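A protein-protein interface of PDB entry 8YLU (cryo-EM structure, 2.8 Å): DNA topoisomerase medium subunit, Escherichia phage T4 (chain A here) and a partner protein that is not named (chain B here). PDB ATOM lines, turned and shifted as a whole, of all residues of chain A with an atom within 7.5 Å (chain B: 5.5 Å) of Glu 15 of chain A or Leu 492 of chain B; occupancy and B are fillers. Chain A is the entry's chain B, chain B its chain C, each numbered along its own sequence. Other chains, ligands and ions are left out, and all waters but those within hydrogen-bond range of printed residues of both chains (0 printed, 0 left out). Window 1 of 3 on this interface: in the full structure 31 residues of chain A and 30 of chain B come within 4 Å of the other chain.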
ATOM      1  N   ARG A   6     -21.523  14.320  14.983  1.00  0.00           N
ATOM      2  CA  ARG A   6     -21.969  15.645  15.396  1.00  0.00           C
ATOM      3  C   ARG A   6     -23.466  15.600  15.644  1.00  0.00           C
ATOM      4  O   ARG A   6     -24.239  15.362  14.713  1.00  0.00           O
ATOM      5  CB  ARG A   6     -21.631  16.693  14.334  1.00  0.00           C
ATOM      6  CG  ARG A   6     -22.091  18.094  14.682  1.00  0.00           C
ATOM      7  CD  ARG A   6     -20.940  18.935  15.203  1.00  0.00           C
ATOM      8  NE  ARG A   6     -21.361  20.286  15.551  1.00  0.00           N
ATOM      9  CZ  ARG A   6     -21.436  21.292  14.692  1.00  0.00           C
ATOM     10  NH1 ARG A   6     -21.129  21.136  13.416  1.00  0.00           N
ATOM     11  NH2 ARG A   6     -21.826  22.488  15.125  1.00  0.00           N
ATOM     12  N   ASP A   7     -23.872  15.828  16.889  1.00  0.00           N
ATOM     13  CA  ASP A   7     -25.286  15.816  17.227  1.00  0.00           C
ATOM     14  C   ASP A   7     -25.998  17.010  16.603  1.00  0.00           C
ATOM     15  O   ASP A   7     -25.391  18.043  16.310  1.00  0.00           O
ATOM     16  CB  ASP A   7     -25.471  15.836  18.743  1.00  0.00           C
ATOM     17  CG  ASP A   7     -26.638  14.989  19.195  1.00  0.00           C
ATOM     18  OD1 ASP A   7     -26.689  13.798  18.825  1.00  0.00           O
ATOM     19  OD2 ASP A   7     -27.506  15.515  19.923  1.00  0.00           O
ATOM     20  N   LEU A   8     -27.307  16.857  16.396  1.00  0.00           N
ATOM     21  CA  LEU A   8     -28.098  17.950  15.842  1.00  0.00           C
ATOM     22  C   LEU A   8     -28.275  19.080  16.846  1.00  0.00           C
ATOM     23  O   LEU A   8     -28.393  20.246  16.449  1.00  0.00           O
ATOM     24  CB  LEU A   8     -29.460  17.431  15.380  1.00  0.00           C
ATOM     25  CG  LEU A   8     -30.449  18.453  14.819  1.00  0.00           C
ATOM     26  CD1 LEU A   8     -30.217  18.670  13.335  1.00  0.00           C
ATOM     27  CD2 LEU A   8     -31.878  18.013  15.081  1.00  0.00           C
ATOM     28  N   LYS A   9     -28.299  18.759  18.142  1.00  0.00           N
ATOM     29  CA  LYS A   9     -28.471  19.793  19.157  1.00  0.00           C
ATOM     30  C   LYS A   9     -27.332  20.803  19.113  1.00  0.00           C
ATOM     31  O   LYS A   9     -27.566  22.014  19.186  1.00  0.00           O
ATOM     32  CB  LYS A   9     -28.576  19.154  20.541  1.00  0.00           C
ATOM     33  CG  LYS A   9     -28.428  20.130  21.693  1.00  0.00           C
ATOM     34  CD  LYS A   9     -29.688  20.953  21.887  1.00  0.00           C
ATOM     35  CE  LYS A   9     -30.155  20.916  23.331  1.00  0.00           C
ATOM     36  NZ  LYS A   9     -31.599  21.253  23.454  1.00  0.00           N
ATOM     37  N   SER A  10     -26.092  20.323  18.983  1.00  0.00           N
ATOM     38  CA  SER A  10     -24.957  21.233  18.870  1.00  0.00           C
ATOM     39  C   SER A  10     -25.018  22.051  17.587  1.00  0.00           C
ATOM     40  O   SER A  10     -24.687  23.241  17.599  1.00  0.00           O
ATOM     41  CB  SER A  10     -23.646  20.453  18.940  1.00  0.00           C
ATOM     42  OG  SER A  10     -23.302  19.919  17.676  1.00  0.00           O
ATOM     43  N   ILE A  11     -25.439  21.436  16.481  1.00  0.00           N
ATOM     44  CA  ILE A  11     -25.590  22.171  15.230  1.00  0.00           C
ATOM     45  C   ILE A  11     -26.569  23.322  15.405  1.00  0.00           C
ATOM     46  O   ILE A  11     -26.278  24.466  15.032  1.00  0.00           O
ATOM     47  CB  ILE A  11     -26.041  21.220  14.106  1.00  0.00           C
ATOM     48  CG1 ILE A  11     -24.994  20.133  13.866  1.00  0.00           C
ATOM     49  CG2 ILE A  11     -26.330  21.994  12.830  1.00  0.00           C
ATOM     50  CD1 ILE A  11     -25.484  19.000  13.004  1.00  0.00           C
ATOM     51  N   ILE A  12     -27.734  23.041  15.992  1.00  0.00           N
ATOM     52  CA  ILE A  12     -28.748  24.074  16.174  1.00  0.00           C
ATOM     53  C   ILE A  12     -28.253  25.153  17.128  1.00  0.00           C
ATOM     54  O   ILE A  12     -28.422  26.350  16.872  1.00  0.00           O
ATOM     55  CB  ILE A  12     -30.064  23.442  16.663  1.00  0.00           C
ATOM     56  CG1 ILE A  12     -30.600  22.467  15.612  1.00  0.00           C
ATOM     57  CG2 ILE A  12     -31.086  24.520  16.983  1.00  0.00           C
ATOM     58  CD1 ILE A  12     -32.068  22.156  15.749  1.00  0.00           C
ATOM     59  N   ASP A  13     -27.625  24.755  18.233  1.00  0.00           N
ATOM     60  CA  ASP A  13     -27.196  25.712  19.240  1.00  0.00           C
ATOM     61  C   ASP A  13     -25.954  26.493  18.840  1.00  0.00           C
ATOM     62  O   ASP A  13     -25.624  27.474  19.514  1.00  0.00           O
ATOM     63  CB  ASP A  13     -26.942  25.000  20.568  1.00  0.00           C
ATOM     64  CG  ASP A  13     -28.217  24.748  21.345  1.00  0.00           C
ATOM     65  OD1 ASP A  13     -29.264  24.504  20.711  1.00  0.00           O
ATOM     66  OD2 ASP A  13     -28.174  24.793  22.592  1.00  0.00           O
ATOM     67  N   ASN A  14     -25.252  26.095  17.779  1.00  0.00           N
ATOM     68  CA  ASN A  14     -24.092  26.855  17.336  1.00  0.00           C
ATOM     69  C   ASN A  14     -24.333  27.572  16.015  1.00  0.00           C
ATOM     70  O   ASN A  14     -24.407  28.802  15.992  1.00  0.00           O
ATOM     71  CB  ASN A  14     -22.882  25.920  17.215  1.00  0.00           C
ATOM     72  CG  ASN A  14     -22.112  25.792  18.509  1.00  0.00           C
ATOM     73  OD1 ASN A  14     -22.536  25.098  19.432  1.00  0.00           O
ATOM     74  ND2 ASN A  14     -20.969  26.462  18.585  1.00  0.00           N
ATOM     75  N   GLU A  15     -24.584  26.845  14.930  1.00  0.00           N
ATOM     76  CA  GLU A  15     -24.645  27.482  13.619  1.00  0.00           C
ATOM     77  C   GLU A  15     -26.003  28.098  13.321  1.00  0.00           C
ATOM     78  O   GLU A  15     -26.069  29.219  12.811  1.00  0.00           O
ATOM     79  CB  GLU A  15     -24.280  26.479  12.522  1.00  0.00           C
ATOM     80  CG  GLU A  15     -22.844  25.991  12.603  1.00  0.00           C
ATOM     81  CD  GLU A  15     -22.748  24.505  12.860  1.00  0.00           C
ATOM     82  OE1 GLU A  15     -23.744  23.799  12.617  1.00  0.00           O
ATOM     83  OE2 GLU A  15     -21.678  24.043  13.307  1.00  0.00           O
ATOM     84  N   ALA A  16     -27.090  27.396  13.643  1.00  0.00           N
ATOM     85  CA  ALA A  16     -28.414  27.986  13.495  1.00  0.00           C
ATOM     86  C   ALA A  16     -28.577  29.198  14.403  1.00  0.00           C
ATOM     87  O   ALA A  16     -29.141  30.218  13.990  1.00  0.00           O
ATOM     88  CB  ALA A  16     -29.487  26.940  13.788  1.00  0.00           C
ATOM     89  N   LEU A  17     -28.083  29.108  15.640  1.00  0.00           N
ATOM     90  CA  LEU A  17     -28.168  30.240  16.556  1.00  0.00           C
ATOM     91  C   LEU A  17     -27.315  31.406  16.075  1.00  0.00           C
ATOM     92  O   LEU A  17     -27.734  32.566  16.165  1.00  0.00           O
ATOM     93  CB  LEU A  17     -27.757  29.813  17.964  1.00  0.00           C
ATOM     94  CG  LEU A  17     -27.972  30.823  19.094  1.00  0.00           C
ATOM     95  CD1 LEU A  17     -29.278  31.574  18.916  1.00  0.00           C
ATOM     96  CD2 LEU A  17     -27.939  30.128  20.440  1.00  0.00           C
ATOM     97  N   ALA A  18     -26.117  31.122  15.554  1.00  0.00           N
ATOM     98  CA  ALA A  18     -25.284  32.186  15.011  1.00  0.00           C
ATOM     99  C   ALA A  18     -25.963  32.868  13.835  1.00  0.00           C
ATOM    100  O   ALA A  18     -25.942  34.097  13.729  1.00  0.00           O
ATOM    101  CB  ALA A  18     -23.923  31.628  14.599  1.00  0.00           C
ATOM    102  N   TYR A  19     -26.583  32.090  12.945  1.00  0.00           N
ATOM    103  CA  TYR A  19     -27.274  32.692  11.809  1.00  0.00           C
ATOM    104  C   TYR A  19     -28.469  33.526  12.254  1.00  0.00           C
ATOM    105  O   TYR A  19     -28.698  34.618  11.723  1.00  0.00           O
ATOM    106  CB  TYR A  19     -27.725  31.620  10.824  1.00  0.00           C
ATOM    107  CG  TYR A  19     -28.620  32.171   9.739  1.00  0.00           C
ATOM    108  CD1 TYR A  19     -28.113  33.008   8.758  1.00  0.00           C
ATOM    109  CD2 TYR A  19     -29.975  31.871   9.709  1.00  0.00           C
ATOM    110  CE1 TYR A  19     -28.923  33.520   7.772  1.00  0.00           C
ATOM    111  CE2 TYR A  19     -30.794  32.381   8.726  1.00  0.00           C
ATOM    112  CZ  TYR A  19     -30.261  33.204   7.760  1.00  0.00           C
ATOM    113  OH  TYR A  19     -31.073  33.716   6.776  1.00  0.00           O
ATOM    114  N   ALA A  20     -29.256  33.024  13.209  1.00  0.00           N
ATOM    115  CA  ALA A  20     -30.420  33.772  13.673  1.00  0.00           C
ATOM    116  C   ALA A  20     -30.004  35.082  14.332  1.00  0.00           C
ATOM    117  O   ALA A  20     -30.578  36.146  14.057  1.00  0.00           O
ATOM    118  CB  ALA A  20     -31.239  32.917  14.638  1.00  0.00           C
ATOM    119  N   MET A  21     -28.988  35.027  15.196  1.00  0.00           N
ATOM    120  CA  MET A  21     -28.521  36.242  15.848  1.00  0.00           C
ATOM    121  C   MET A  21     -27.878  37.192  14.848  1.00  0.00           C
ATOM    122  O   MET A  21     -27.972  38.410  15.011  1.00  0.00           O
ATOM    123  CB  MET A  21     -27.542  35.894  16.969  1.00  0.00           C
ATOM    124  CG  MET A  21     -28.202  35.403  18.260  1.00  0.00           C
ATOM    125  SD  MET A  21     -29.480  36.433  19.020  1.00  0.00           S
ATOM    126  CE  MET A  21     -28.884  38.094  18.724  1.00  0.00           C
ATOM    127  N   THR B 485     -22.188  22.951   1.707  1.00  0.00           N
ATOM    128  CA  THR B 485     -22.673  24.287   1.407  1.00  0.00           C
ATOM    129  C   THR B 485     -21.604  25.319   1.739  1.00  0.00           C
ATOM    130  O   THR B 485     -20.560  25.011   2.317  1.00  0.00           O
ATOM    131  CB  THR B 485     -23.956  24.580   2.193  1.00  0.00           C
ATOM    132  OG1 THR B 485     -23.775  24.199   3.562  1.00  0.00           O
ATOM    133  CG2 THR B 485     -25.125  23.802   1.618  1.00  0.00           C
ATOM    134  N   ASP B 486     -21.879  26.562   1.357  1.00  0.00           N
ATOM    135  CA  ASP B 486     -20.986  27.655   1.707  1.00  0.00           C
ATOM    136  C   ASP B 486     -20.940  27.823   3.222  1.00  0.00           C
ATOM    137  O   ASP B 486     -21.923  27.583   3.926  1.00  0.00           O
ATOM    138  CB  ASP B 486     -21.442  28.948   1.034  1.00  0.00           C
ATOM    139  CG  ASP B 486     -21.766  28.758  -0.435  1.00  0.00           C
ATOM    140  OD1 ASP B 486     -21.396  27.708  -0.998  1.00  0.00           O
ATOM    141  OD2 ASP B 486     -22.385  29.664  -1.030  1.00  0.00           O
ATOM    142  N   ALA B 487     -19.778  28.228   3.725  1.00  0.00           N
ATOM    143  CA  ALA B 487     -19.518  28.236   5.157  1.00  0.00           C
ATOM    144  C   ALA B 487     -19.894  29.548   5.832  1.00  0.00           C
ATOM    145  O   ALA B 487     -19.640  29.704   7.030  1.00  0.00           O
ATOM    146  CB  ALA B 487     -18.046  27.921   5.426  1.00  0.00           C
ATOM    147  N   ASP B 488     -20.491  30.490   5.106  1.00  0.00           N
ATOM    148  CA  ASP B 488     -20.947  31.718   5.736  1.00  0.00           C
ATOM    149  C   ASP B 488     -22.203  31.443   6.559  1.00  0.00           C
ATOM    150  O   ASP B 488     -22.651  30.304   6.704  1.00  0.00           O
ATOM    151  CB  ASP B 488     -21.201  32.801   4.691  1.00  0.00           C
ATOM    152  CG  ASP B 488     -22.056  32.318   3.549  1.00  0.00           C
ATOM    153  OD1 ASP B 488     -21.774  31.226   3.027  1.00  0.00           O
ATOM    154  OD2 ASP B 488     -23.009  33.029   3.169  1.00  0.00           O
ATOM    155  N   HIS B 489     -22.779  32.511   7.112  1.00  0.00           N
ATOM    156  CA  HIS B 489     -23.902  32.351   8.029  1.00  0.00           C
ATOM    157  C   HIS B 489     -25.119  31.754   7.335  1.00  0.00           C
ATOM    158  O   HIS B 489     -25.776  30.863   7.883  1.00  0.00           O
ATOM    159  CB  HIS B 489     -24.249  33.697   8.663  1.00  0.00           C
ATOM    160  CG  HIS B 489     -23.308  34.108   9.751  1.00  0.00           C
ATOM    161  ND1 HIS B 489     -22.352  35.086   9.576  1.00  0.00           N
ATOM    162  CD2 HIS B 489     -23.165  33.666  11.022  1.00  0.00           C
ATOM    163  CE1 HIS B 489     -21.667  35.233  10.695  1.00  0.00           C
ATOM    164  NE2 HIS B 489     -22.140  34.383  11.587  1.00  0.00           N
ATOM    165  N   ASP B 490     -25.433  32.226   6.126  1.00  0.00           N
ATOM    166  CA  ASP B 490     -26.629  31.751   5.436  1.00  0.00           C
ATOM    167  C   ASP B 490     -26.519  30.272   5.087  1.00  0.00           C
ATOM    168  O   ASP B 490     -27.446  29.494   5.337  1.00  0.00           O
ATOM    169  CB  ASP B 490     -26.874  32.582   4.178  1.00  0.00           C
ATOM    170  CG  ASP B 490     -27.224  34.020   4.491  1.00  0.00           C
ATOM    171  OD1 ASP B 490     -26.319  34.780   4.895  1.00  0.00           O
ATOM    172  OD2 ASP B 490     -28.404  34.390   4.336  1.00  0.00           O
ATOM    173  N   GLY B 491     -25.391  29.865   4.506  1.00  0.00           N
ATOM    174  CA  GLY B 491     -25.226  28.474   4.125  1.00  0.00           C
ATOM    175  C   GLY B 491     -25.150  27.529   5.304  1.00  0.00           C
ATOM    176  O   GLY B 491     -25.599  26.383   5.215  1.00  0.00           O
ATOM    177  N   LEU B 492     -24.588  27.986   6.419  1.00  0.00           N
ATOM    178  CA  LEU B 492     -24.317  27.118   7.555  1.00  0.00           C
ATOM    179  C   LEU B 492     -25.444  27.082   8.578  1.00  0.00           C
ATOM    180  O   LEU B 492     -25.564  26.090   9.306  1.00  0.00           O
ATOM    181  CB  LEU B 492     -23.025  27.564   8.245  1.00  0.00           C
ATOM    182  CG  LEU B 492     -22.253  26.541   9.075  1.00  0.00           C
ATOM    183  CD1 LEU B 492     -22.353  25.162   8.462  1.00  0.00           C
ATOM    184  CD2 LEU B 492     -20.805  26.969   9.201  1.00  0.00           C
ATOM    185  N   GLY B 493     -26.266  28.124   8.659  1.00  0.00           N
ATOM    186  CA  GLY B 493     -27.290  28.183   9.682  1.00  0.00           C
ATOM    187  C   GLY B 493     -28.706  28.237   9.152  1.00  0.00           C
ATOM    188  O   GLY B 493     -29.662  28.175   9.929  1.00  0.00           O
ATOM    189  N   SER B 494     -28.860  28.369   7.835  1.00  0.00           N
ATOM    190  CA  SER B 494     -30.178  28.353   7.212  1.00  0.00           C
ATOM    191  C   SER B 494     -30.355  27.161   6.284  1.00  0.00           C
ATOM    192  O   SER B 494     -31.291  26.377   6.466  1.00  0.00           O
ATOM    193  CB  SER B 494     -30.416  29.663   6.453  1.00  0.00           C
ATOM    194  OG  SER B 494     -31.770  29.785   6.056  1.00  0.00           O
ATOM    195  N   ILE B 495     -29.479  27.000   5.291  1.00  0.00           N
ATOM    196  CA  ILE B 495     -29.654  25.944   4.301  1.00  0.00           C
ATOM    197  C   ILE B 495     -29.326  24.581   4.899  1.00  0.00           C
ATOM    198  O   ILE B 495     -30.021  23.593   4.639  1.00  0.00           O
ATOM    199  CB  ILE B 495     -28.800  26.248   3.058  1.00  0.00           C
ATOM    200  CG1 ILE B 495     -29.211  27.594   2.460  1.00  0.00           C
ATOM    201  CG2 ILE B 495     -28.930  25.146   2.028  1.00  0.00           C
ATOM    202  CD1 ILE B 495     -28.293  28.092   1.380  1.00  0.00           C
ATOM    203  N   TYR B 496     -28.265  24.503   5.697  1.00  0.00           N
ATOM    204  CA  TYR B 496     -27.855  23.223   6.272  1.00  0.00           C
ATOM    205  C   TYR B 496     -28.888  22.641   7.234  1.00  0.00           C
ATOM    206  O   TYR B 496     -29.255  21.462   7.070  1.00  0.00           O
ATOM    207  CB  TYR B 496     -26.473  23.403   6.916  1.00  0.00           C
ATOM    208  CG  TYR B 496     -25.915  22.207   7.650  1.00  0.00           C
ATOM    209  CD1 TYR B 496     -26.167  20.911   7.219  1.00  0.00           C
ATOM    210  CD2 TYR B 496     -25.119  22.379   8.771  1.00  0.00           C
ATOM    211  CE1 TYR B 496     -25.650  19.825   7.895  1.00  0.00           C
ATOM    212  CE2 TYR B 496     -24.599  21.302   9.450  1.00  0.00           C
ATOM    213  CZ  TYR B 496     -24.866  20.027   9.007  1.00  0.00           C
ATOM    214  OH  TYR B 496     -24.346  18.953   9.686  1.00  0.00           O
ATOM    215  N   PRO B 497     -29.401  23.373   8.234  1.00  0.00           N
ATOM    216  CA  PRO B 497     -30.425  22.769   9.102  1.00  0.00           C
ATOM    217  C   PRO B 497     -31.745  22.514   8.395  1.00  0.00           C
ATOM    218  O   PRO B 497     -32.446  21.560   8.751  1.00  0.00           O
ATOM    219  CB  PRO B 497     -30.577  23.792  10.234  1.00  0.00           C
ATOM    220  CG  PRO B 497     -30.128  25.063   9.651  1.00  0.00           C
ATOM    221  CD  PRO B 497     -29.029  24.720   8.703  1.00  0.00           C
ATOM    222  N   PHE B 517     -21.730  16.215   6.544  1.00  0.00           N
ATOM    223  CA  PHE B 517     -21.484  17.603   6.182  1.00  0.00           C
ATOM    224  C   PHE B 517     -20.000  17.779   5.905  1.00  0.00           C
ATOM    225  O   PHE B 517     -19.163  17.408   6.732  1.00  0.00           O
ATOM    226  CB  PHE B 517     -21.931  18.561   7.287  1.00  0.00           C
ATOM    227  CG  PHE B 517     -21.697  20.005   6.958  1.00  0.00           C
ATOM    228  CD1 PHE B 517     -22.423  20.626   5.958  1.00  0.00           C
ATOM    229  CD2 PHE B 517     -20.746  20.739   7.640  1.00  0.00           C
ATOM    230  CE1 PHE B 517     -22.209  21.949   5.649  1.00  0.00           C
ATOM    231  CE2 PHE B 517     -20.529  22.061   7.335  1.00  0.00           C
ATOM    232  CZ  PHE B 517     -21.260  22.666   6.337  1.00  0.00           C
ATOM    233  N   TYR B 535     -13.049  27.198   9.795  1.00  0.00           N
ATOM    234  CA  TYR B 535     -14.292  26.720   9.202  1.00  0.00           C
ATOM    235  C   TYR B 535     -15.484  27.599   9.555  1.00  0.00           C
ATOM    236  O   TYR B 535     -16.398  27.748   8.738  1.00  0.00           O
ATOM    237  CB  TYR B 535     -14.543  25.275   9.631  1.00  0.00           C
ATOM    238  CG  TYR B 535     -13.501  24.318   9.102  1.00  0.00           C
ATOM    239  CD1 TYR B 535     -12.978  24.475   7.828  1.00  0.00           C
ATOM    240  CD2 TYR B 535     -13.034  23.268   9.877  1.00  0.00           C
ATOM    241  CE1 TYR B 535     -12.026  23.613   7.336  1.00  0.00           C
ATOM    242  CE2 TYR B 535     -12.080  22.397   9.392  1.00  0.00           C
ATOM    243  CZ  TYR B 535     -11.579  22.575   8.120  1.00  0.00           C
ATOM    244  OH  TYR B 535     -10.628  21.714   7.629  1.00  0.00           O
ATOM    245  N   THR B 536     -15.498  28.182  10.749  1.00  0.00           N
ATOM    246  CA  THR B 536     -16.565  29.075  11.170  1.00  0.00           C
ATOM    247  C   THR B 536     -15.981  30.425  11.559  1.00  0.00           C
ATOM    248  O   THR B 536     -14.824  30.522  11.977  1.00  0.00           O
ATOM    249  CB  THR B 536     -17.358  28.492  12.345  1.00  0.00           C
ATOM    250  OG1 THR B 536     -16.463  28.154  13.408  1.00  0.00           O
ATOM    251  CG2 THR B 536     -18.111  27.247  11.910  1.00  0.00           C
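Printed residues of chain B that touch a printed residue of chain A: His 489, Asp 490, Leu 492, Gly 493, Ser 494 and Tyr 496. Hydrophobic or aromatic side chains of chain B that line the printed part of chain A: His 489, Leu 492 and Tyr 496. Along chain B the printed residues that touch a printed residue of chain A span positions 489 to 496. Of the 16 printed residues of chain A, 5 touch a printed residue of chain B. Printed residues of chain A that touch a printed residue of chain B: Ile 11, Glu 15, Ala 16, Ala 18 and Tyr 19. Hydrophobic or aromatic side chains of chain A that line the printed part of chain B: Ile 11 and Tyr 19. Among the printed residues, no Asp or Glu carboxylate lies within 4 Å of a Lys or Arg side-chain nitrogen of the other chain.
Lys 9 of chain A touches none of the printed residues of chain B. Glu 15 of chain A touches just these residues of chain B: Leu 492 and Gly 493. Of the printed residues of chain B, Tyr 19 of chain A touches His 489 (3.3 Å), Asp 490 (3.6 Å), Gly 493 (3.6 Å) and Ser 494 (3.6 Å). Printed residues of chain A within 4 Å of His 489 of chain B: Ala 18 and Tyr 19. Of the printed residues of chain A, Asp 490 of chain B touches Tyr 19. Leu 492 of chain B touches one residue of chain A. Of the printed residues of chain A, Tyr 496 of chain B touches Ile 11. The nearest residue of chain B that does not touch Glu 15 of chain A is Tyr 496 of chain B (4.1 Å). The nearest printed residue of chain A that does not touch His 489 of chain B is Glu 15 of chain A (5.2 Å).
The side-chain carboxylate (OE2) of Glu 15 of chain A is in salt-bridge range of the guanidinium group (NH1) of Arg 6 of chain A (3.0 Å). The backbone NH (N) of Ala 16 of chain A sits at hydrogen-bond distance from the backbone carbonyl oxygen (O) of Ile 11 of chain A (3.3 Å). N of Ile 495 of chain B lies within hydrogen-bond range of O of Asp 490 of chain B, at 3.2 Å. O of Gly 491 of chain B is in hydrogen-bond range of N of Tyr 496 of chain B (3.3 Å).
Among the printed residues, merely in contact across the chains: Ile 11 of chain A with Tyr 496 of chain B (3.5 Å), Glu 15 of chain A with Leu 492 of chain B (3.5 Å), Glu 15 of chain A with Gly 493 of chain B (3.5 Å), Ala 16 of chain A with Gly 493 of chain B (3.8 Å), Ala 18 of chain A with His 489 of chain B (3.9 Å), Tyr 19 of chain A with His 489 of chain B (3.3 Å), Tyr 19 of chain A with Asp 490 of chain B (3.6 Å), Tyr 19 of chain A with Gly 493 of chain B (3.6 Å) and Tyr 19 of chain A with Ser 494 of chain B (3.6 Å).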
